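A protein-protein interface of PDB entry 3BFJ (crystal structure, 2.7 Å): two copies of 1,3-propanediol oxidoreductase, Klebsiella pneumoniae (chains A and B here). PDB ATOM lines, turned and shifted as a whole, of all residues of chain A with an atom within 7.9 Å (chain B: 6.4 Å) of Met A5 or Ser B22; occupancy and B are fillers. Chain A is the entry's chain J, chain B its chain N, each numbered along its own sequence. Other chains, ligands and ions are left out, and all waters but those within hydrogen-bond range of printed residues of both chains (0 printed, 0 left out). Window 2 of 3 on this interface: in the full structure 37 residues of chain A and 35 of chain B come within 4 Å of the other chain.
The backbone carbonyl oxygen (O) of Phe B16 is in hydrogen-bond range of the backbone NH (N) of Phe A6 (2.8 Å).
O of Asn B19 sits at hydrogen-bond distance from OG of Ser B22, 2.9 Å away. N of Ala B20 is in hydrogen-bond range of OD1 of Asp B180 (2.9 Å). The backbone NH (N) of Asn B19 lies within hydrogen-bond range of the side-chain carboxylate (OD2) of Asp B180 (2.9 Å).
CA of Gly B17 touches O of Arg A4 (3.8 Å). Arg A4 touches Pro B18 (O to CD, 3.2 Å). Met A5 touches Phe B16 (CG to O, 3.6 Å). CB of Met A5 touches O of Pro B18, 3.8 Å away. O of Asn B19 touches CE of Met A5 (3.5 Å). Met A5 touches Ala B20. OG of Ser B22 touches CE of Met A5 (3.5 Å). O of Phe A6 touches CA of Phe B15 (3.4 Å). CB of Asp A7 touches CE2 of Phe B15, 3.4 Å away. Phe B16 touches Asn A213.
Of the printed residues of chain B, Arg A4 touches Gly B17 (3.8 Å) and Pro B18 (3.2 Å). Printed residues of chain B within 4 Å of Asp A7: Phe B15. Of the printed residues of chain A, Phe B15 touches Phe A6 and Asp A7. Of the printed residues of chain A, Phe B16 touches Met A5 (3.6 Å), Phe A6 (2.8 Å) and Asn A213 (3.7 Å). Of the printed residues of chain A, Gly B17 touches Arg A4. Ser B22 touches one residue of chain A. Glu B26 touches none of the printed residues of chain A. The nearest printed residue of chain B that does not touch Met A5 is Gly B17 (4.3 Å). The nearest printed residue of chain A that does not touch Phe B15 is Met A5 (4.3 Å).
Of the 6 printed residues of chain A, 5 touch a printed residue of chain B. Hydrophobic or aromatic side chains of chain A within 4 Å of the printed part of chain B: Met A5 and Phe A6. Of the 15 printed residues of chain B, 7 touch a printed residue of chain A. Hydrophobic or aromatic side chains of chain B within 4 Å of the printed part of chain A: Phe B15, Phe B16, Pro B18 and Ala B20. Among the printed residues, 11 pairs touch across the chains. Among the printed residues, no Asp or Glu carboxylate lies within 4 Å of a Lys or Arg side-chain nitrogen of the other chain.
No position is printed for both chains. Of the 11 pairs that touch across the chains among the printed residues, none has its exchanged pair printed and touching as well.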
ATOM      1  N   ARG A   4      -6.166  -7.844 -16.959  1.00  0.00           N
ATOM      2  CA  ARG A   4      -6.882  -8.122 -15.676  1.00  0.00           C
ATOM      3  C   ARG A   4      -5.905  -8.264 -14.506  1.00  0.00           C
ATOM      4  O   ARG A   4      -6.228  -7.882 -13.381  1.00  0.00           O
ATOM      5  CB  ARG A   4      -7.780  -9.366 -15.797  1.00  0.00           C
ATOM      6  CG  ARG A   4      -7.022 -10.694 -15.909  1.00  0.00           C
ATOM      7  CD  ARG A   4      -7.925 -11.918 -15.779  1.00  0.00           C
ATOM      8  NE  ARG A   4      -8.817 -11.848 -14.620  1.00  0.00           N
ATOM      9  CZ  ARG A   4     -10.144 -11.746 -14.695  1.00  0.00           C
ATOM     10  NH1 ARG A   4     -10.749 -11.713 -15.878  1.00  0.00           N
ATOM     11  NH2 ARG A   4     -10.869 -11.687 -13.584  1.00  0.00           N
ATOM     12  N   MET A   5      -4.721  -8.809 -14.792  1.00  0.00           N
ATOM     13  CA  MET A   5      -3.649  -8.990 -13.813  1.00  0.00           C
ATOM     14  C   MET A   5      -2.374  -8.311 -14.311  1.00  0.00           C
ATOM     15  O   MET A   5      -2.124  -8.265 -15.515  1.00  0.00           O
ATOM     16  CB  MET A   5      -3.393 -10.479 -13.606  1.00  0.00           C
ATOM     17  CG  MET A   5      -2.283 -10.826 -12.609  1.00  0.00           C
ATOM     18  SD  MET A   5      -1.281 -12.254 -13.117  1.00  0.00           S
ATOM     19  CE  MET A   5      -2.521 -13.488 -13.528  1.00  0.00           C
ATOM     20  N   PHE A   6      -1.563  -7.795 -13.392  1.00  0.00           N
ATOM     21  CA  PHE A   6      -0.367  -7.045 -13.772  1.00  0.00           C
ATOM     22  C   PHE A   6       0.863  -7.469 -12.987  1.00  0.00           C
ATOM     23  O   PHE A   6       0.763  -7.921 -11.843  1.00  0.00           O
ATOM     24  CB  PHE A   6      -0.575  -5.538 -13.579  1.00  0.00           C
ATOM     25  CG  PHE A   6      -1.919  -5.046 -14.012  1.00  0.00           C
ATOM     26  CD1 PHE A   6      -2.130  -4.624 -15.317  1.00  0.00           C
ATOM     27  CD2 PHE A   6      -2.982  -5.006 -13.110  1.00  0.00           C
ATOM     28  CE1 PHE A   6      -3.384  -4.170 -15.723  1.00  0.00           C
ATOM     29  CE2 PHE A   6      -4.237  -4.555 -13.503  1.00  0.00           C
ATOM     30  CZ  PHE A   6      -4.438  -4.135 -14.815  1.00  0.00           C
ATOM     31  N   ASP A   7       2.022  -7.315 -13.619  1.00  0.00           N
ATOM     32  CA  ASP A   7       3.300  -7.417 -12.926  1.00  0.00           C
ATOM     33  C   ASP A   7       3.953  -6.042 -12.804  1.00  0.00           C
ATOM     34  O   ASP A   7       3.705  -5.148 -13.615  1.00  0.00           O
ATOM     35  CB  ASP A   7       4.240  -8.390 -13.635  1.00  0.00           C
ATOM     36  CG  ASP A   7       4.585  -7.949 -15.039  1.00  0.00           C
ATOM     37  OD1 ASP A   7       3.792  -8.232 -15.965  1.00  0.00           O
ATOM     38  OD2 ASP A   7       5.648  -7.318 -15.212  1.00  0.00           O
ATOM     39  N   ASP A 211      -2.235  -0.734 -20.554  1.00  0.00           N
ATOM     40  CA  ASP A 211      -1.746  -1.516 -19.420  1.00  0.00           C
ATOM     41  C   ASP A 211      -1.593  -0.681 -18.138  1.00  0.00           C
ATOM     42  O   ASP A 211      -1.110  -1.168 -17.114  1.00  0.00           O
ATOM     43  CB  ASP A 211      -0.419  -2.174 -19.794  1.00  0.00           C
ATOM     44  CG  ASP A 211      -0.523  -3.005 -21.058  1.00  0.00           C
ATOM     45  OD1 ASP A 211      -1.577  -3.655 -21.251  1.00  0.00           O
ATOM     46  OD2 ASP A 211       0.447  -3.010 -21.853  1.00  0.00           O
ATOM     47  N   ASN A 213      -2.442   0.904 -14.692  1.00  0.00           N
ATOM     48  CA  ASN A 213      -3.160   0.504 -13.482  1.00  0.00           C
ATOM     49  C   ASN A 213      -2.901   1.536 -12.373  1.00  0.00           C
ATOM     50  O   ASN A 213      -1.982   2.354 -12.501  1.00  0.00           O
ATOM     51  CB  ASN A 213      -2.750  -0.915 -13.040  1.00  0.00           C
ATOM     52  CG  ASN A 213      -1.239  -1.074 -12.833  1.00  0.00           C
ATOM     53  OD1 ASN A 213      -0.584  -1.825 -13.553  1.00  0.00           O
ATOM     54  ND2 ASN A 213      -0.695  -0.391 -11.838  1.00  0.00           N
ATOM     55  N   PHE B  15       3.373  -9.034  -8.382  1.00  0.00           N
ATOM     56  CA  PHE B  15       2.145  -9.319  -9.119  1.00  0.00           C
ATOM     57  C   PHE B  15       0.931  -8.857  -8.333  1.00  0.00           C
ATOM     58  O   PHE B  15       0.850  -9.071  -7.121  1.00  0.00           O
ATOM     59  CB  PHE B  15       2.029 -10.811  -9.424  1.00  0.00           C
ATOM     60  CG  PHE B  15       2.990 -11.291 -10.468  1.00  0.00           C
ATOM     61  CD1 PHE B  15       4.212 -11.841 -10.104  1.00  0.00           C
ATOM     62  CD2 PHE B  15       2.668 -11.203 -11.818  1.00  0.00           C
ATOM     63  CE1 PHE B  15       5.107 -12.288 -11.068  1.00  0.00           C
ATOM     64  CE2 PHE B  15       3.555 -11.651 -12.791  1.00  0.00           C
ATOM     65  CZ  PHE B  15       4.781 -12.187 -12.415  1.00  0.00           C
ATOM     66  N   PHE B  16      -0.002  -8.214  -9.027  1.00  0.00           N
ATOM     67  CA  PHE B  16      -1.267  -7.794  -8.426  1.00  0.00           C
ATOM     68  C   PHE B  16      -2.380  -7.803  -9.469  1.00  0.00           C
ATOM     69  O   PHE B  16      -2.112  -7.804 -10.673  1.00  0.00           O
ATOM     70  CB  PHE B  16      -1.137  -6.413  -7.772  1.00  0.00           C
ATOM     71  CG  PHE B  16      -0.490  -5.383  -8.649  1.00  0.00           C
ATOM     72  CD1 PHE B  16       0.855  -5.069  -8.492  1.00  0.00           C
ATOM     73  CD2 PHE B  16      -1.224  -4.724  -9.637  1.00  0.00           C
ATOM     74  CE1 PHE B  16       1.456  -4.117  -9.307  1.00  0.00           C
ATOM     75  CE2 PHE B  16      -0.633  -3.776 -10.453  1.00  0.00           C
ATOM     76  CZ  PHE B  16       0.705  -3.470 -10.294  1.00  0.00           C
ATOM     77  N   GLY B  17      -3.622  -7.803  -8.993  1.00  0.00           N
ATOM     78  CA  GLY B  17      -4.796  -7.925  -9.853  1.00  0.00           C
ATOM     79  C   GLY B  17      -5.505  -9.241  -9.593  1.00  0.00           C
ATOM     80  O   GLY B  17      -4.912 -10.163  -9.037  1.00  0.00           O
ATOM     81  N   PRO B  18      -6.790  -9.338  -9.967  1.00  0.00           N
ATOM     82  CA  PRO B  18      -7.527 -10.591  -9.820  1.00  0.00           C
ATOM     83  C   PRO B  18      -6.831 -11.786 -10.487  1.00  0.00           C
ATOM     84  O   PRO B  18      -6.351 -11.680 -11.622  1.00  0.00           O
ATOM     85  CB  PRO B  18      -8.867 -10.297 -10.507  1.00  0.00           C
ATOM     86  CG  PRO B  18      -8.649  -9.039 -11.290  1.00  0.00           C
ATOM     87  CD  PRO B  18      -7.638  -8.273 -10.526  1.00  0.00           C
ATOM     88  N   ASN B  19      -6.785 -12.900  -9.761  1.00  0.00           N
ATOM     89  CA  ASN B  19      -6.170 -14.162 -10.205  1.00  0.00           C
ATOM     90  C   ASN B  19      -4.636 -14.184 -10.245  1.00  0.00           C
ATOM     91  O   ASN B  19      -4.036 -15.075 -10.859  1.00  0.00           O
ATOM     92  CB  ASN B  19      -6.761 -14.641 -11.539  1.00  0.00           C
ATOM     93  CG  ASN B  19      -6.707 -16.148 -11.686  1.00  0.00           C
ATOM     94  OD1 ASN B  19      -6.908 -16.888 -10.718  1.00  0.00           O
ATOM     95  ND2 ASN B  19      -6.431 -16.610 -12.896  1.00  0.00           N
ATOM     96  N   ALA B  20      -4.007 -13.229  -9.561  1.00  0.00           N
ATOM     97  CA  ALA B  20      -2.548 -13.131  -9.527  1.00  0.00           C
ATOM     98  C   ALA B  20      -1.898 -14.307  -8.788  1.00  0.00           C
ATOM     99  O   ALA B  20      -0.679 -14.459  -8.806  1.00  0.00           O
ATOM    100  CB  ALA B  20      -2.118 -11.810  -8.914  1.00  0.00           C
ATOM    101  N   ILE B  21      -2.719 -15.133  -8.148  1.00  0.00           N
ATOM    102  CA  ILE B  21      -2.250 -16.349  -7.487  1.00  0.00           C
ATOM    103  C   ILE B  21      -1.713 -17.376  -8.495  1.00  0.00           C
ATOM    104  O   ILE B  21      -0.857 -18.195  -8.161  1.00  0.00           O
ATOM    105  CB  ILE B  21      -3.365 -16.973  -6.576  1.00  0.00           C
ATOM    106  CG1 ILE B  21      -2.779 -17.963  -5.561  1.00  0.00           C
ATOM    107  CG2 ILE B  21      -4.488 -17.609  -7.406  1.00  0.00           C
ATOM    108  CD1 ILE B  21      -1.842 -17.336  -4.552  1.00  0.00           C
ATOM    109  N   SER B  22      -2.200 -17.297  -9.733  1.00  0.00           N
ATOM    110  CA  SER B  22      -1.915 -18.302 -10.761  1.00  0.00           C
ATOM    111  C   SER B  22      -0.441 -18.386 -11.172  1.00  0.00           C
ATOM    112  O   SER B  22      -0.046 -19.330 -11.871  1.00  0.00           O
ATOM    113  CB  SER B  22      -2.808 -18.086 -11.990  1.00  0.00           C
ATOM    114  OG  SER B  22      -2.523 -16.855 -12.629  1.00  0.00           O
ATOM    115  N   VAL B  23       0.366 -17.424 -10.725  1.00  0.00           N
ATOM    116  CA  VAL B  23       1.790 -17.417 -11.062  1.00  0.00           C
ATOM    117  C   VAL B  23       2.735 -18.019 -10.008  1.00  0.00           C
ATOM    118  O   VAL B  23       3.912 -18.217 -10.310  1.00  0.00           O
ATOM    119  CB  VAL B  23       2.308 -16.005 -11.503  1.00  0.00           C
ATOM    120  CG1 VAL B  23       1.669 -15.574 -12.818  1.00  0.00           C
ATOM    121  CG2 VAL B  23       2.089 -14.959 -10.415  1.00  0.00           C
ATOM    122  N   VAL B  24       2.233 -18.320  -8.801  1.00  0.00           N
ATOM    123  CA  VAL B  24       3.096 -18.788  -7.685  1.00  0.00           C
ATOM    124  C   VAL B  24       3.990 -19.966  -8.049  1.00  0.00           C
ATOM    125  O   VAL B  24       5.194 -19.935  -7.787  1.00  0.00           O
ATOM    126  CB  VAL B  24       2.334 -19.155  -6.358  1.00  0.00           C
ATOM    127  CG1 VAL B  24       1.983 -17.922  -5.565  1.00  0.00           C
ATOM    128  CG2 VAL B  24       1.107 -20.035  -6.614  1.00  0.00           C
ATOM    129  N   GLY B  25       3.389 -20.997  -8.640  1.00  0.00           N
ATOM    130  CA  GLY B  25       4.119 -22.187  -9.048  1.00  0.00           C
ATOM    131  C   GLY B  25       5.174 -21.854 -10.080  1.00  0.00           C
ATOM    132  O   GLY B  25       6.336 -22.230  -9.931  1.00  0.00           O
ATOM    133  N   GLU B  26       4.756 -21.130 -11.119  1.00  0.00           N
ATOM    134  CA  GLU B  26       5.642 -20.701 -12.199  1.00  0.00           C
ATOM    135  C   GLU B  26       6.802 -19.869 -11.650  1.00  0.00           C
ATOM    136  O   GLU B  26       7.946 -20.021 -12.082  1.00  0.00           O
ATOM    137  CB  GLU B  26       4.852 -19.911 -13.255  1.00  0.00           C
ATOM    138  CG  GLU B  26       5.523 -19.824 -14.635  1.00  0.00           C
ATOM    139  CD  GLU B  26       4.932 -18.732 -15.544  1.00  0.00           C
ATOM    140  OE1 GLU B  26       4.425 -17.705 -15.030  1.00  0.00           O
ATOM    141  OE2 GLU B  26       4.992 -18.903 -16.785  1.00  0.00           O
ATOM    142  N   TYR B  58      -1.647 -24.421  -7.499  1.00  0.00           N
ATOM    143  CA  TYR B  58      -0.763 -23.950  -8.572  1.00  0.00           C
ATOM    144  C   TYR B  58       0.687 -24.380  -8.367  1.00  0.00           C
ATOM    145  O   TYR B  58       1.461 -24.475  -9.326  1.00  0.00           O
ATOM    146  CB  TYR B  58      -0.848 -22.429  -8.735  1.00  0.00           C
ATOM    147  CG  TYR B  58      -2.159 -21.942  -9.314  1.00  0.00           C
ATOM    148  CD1 TYR B  58      -3.129 -21.365  -8.497  1.00  0.00           C
ATOM    149  CD2 TYR B  58      -2.432 -22.058 -10.678  1.00  0.00           C
ATOM    150  CE1 TYR B  58      -4.334 -20.921  -9.019  1.00  0.00           C
ATOM    151  CE2 TYR B  58      -3.637 -21.617 -11.210  1.00  0.00           C
ATOM    152  CZ  TYR B  58      -4.581 -21.049 -10.373  1.00  0.00           C
ATOM    153  OH  TYR B  58      -5.775 -20.603 -10.885  1.00  0.00           O
ATOM    154  N   ILE B 178       2.746 -11.126  -4.097  1.00  0.00           N
ATOM    155  CA  ILE B 178       1.500 -11.337  -4.833  1.00  0.00           C
ATOM    156  C   ILE B 178       0.302 -10.785  -4.058  1.00  0.00           C
ATOM    157  O   ILE B 178       0.078 -11.147  -2.896  1.00  0.00           O
ATOM    158  CB  ILE B 178       1.300 -12.827  -5.213  1.00  0.00           C
ATOM    159  CG1 ILE B 178       2.317 -13.231  -6.284  1.00  0.00           C
ATOM    160  CG2 ILE B 178      -0.135 -13.074  -5.722  1.00  0.00           C
ATOM    161  CD1 ILE B 178       2.793 -14.653  -6.200  1.00  0.00           C
ATOM    162  N   ASP B 180      -3.525 -10.657  -4.676  1.00  0.00           N
ATOM    163  CA  ASP B 180      -4.703 -11.118  -5.397  1.00  0.00           C
ATOM    164  C   ASP B 180      -5.967 -10.742  -4.620  1.00  0.00           C
ATOM    165  O   ASP B 180      -6.285 -11.373  -3.606  1.00  0.00           O
ATOM    166  CB  ASP B 180      -4.616 -12.639  -5.582  1.00  0.00           C
ATOM    167  CG  ASP B 180      -5.586 -13.177  -6.625  1.00  0.00           C
ATOM    168  OD1 ASP B 180      -5.276 -14.241  -7.195  1.00  0.00           O
ATOM    169  OD2 ASP B 180      -6.648 -12.560  -6.872  1.00  0.00           O
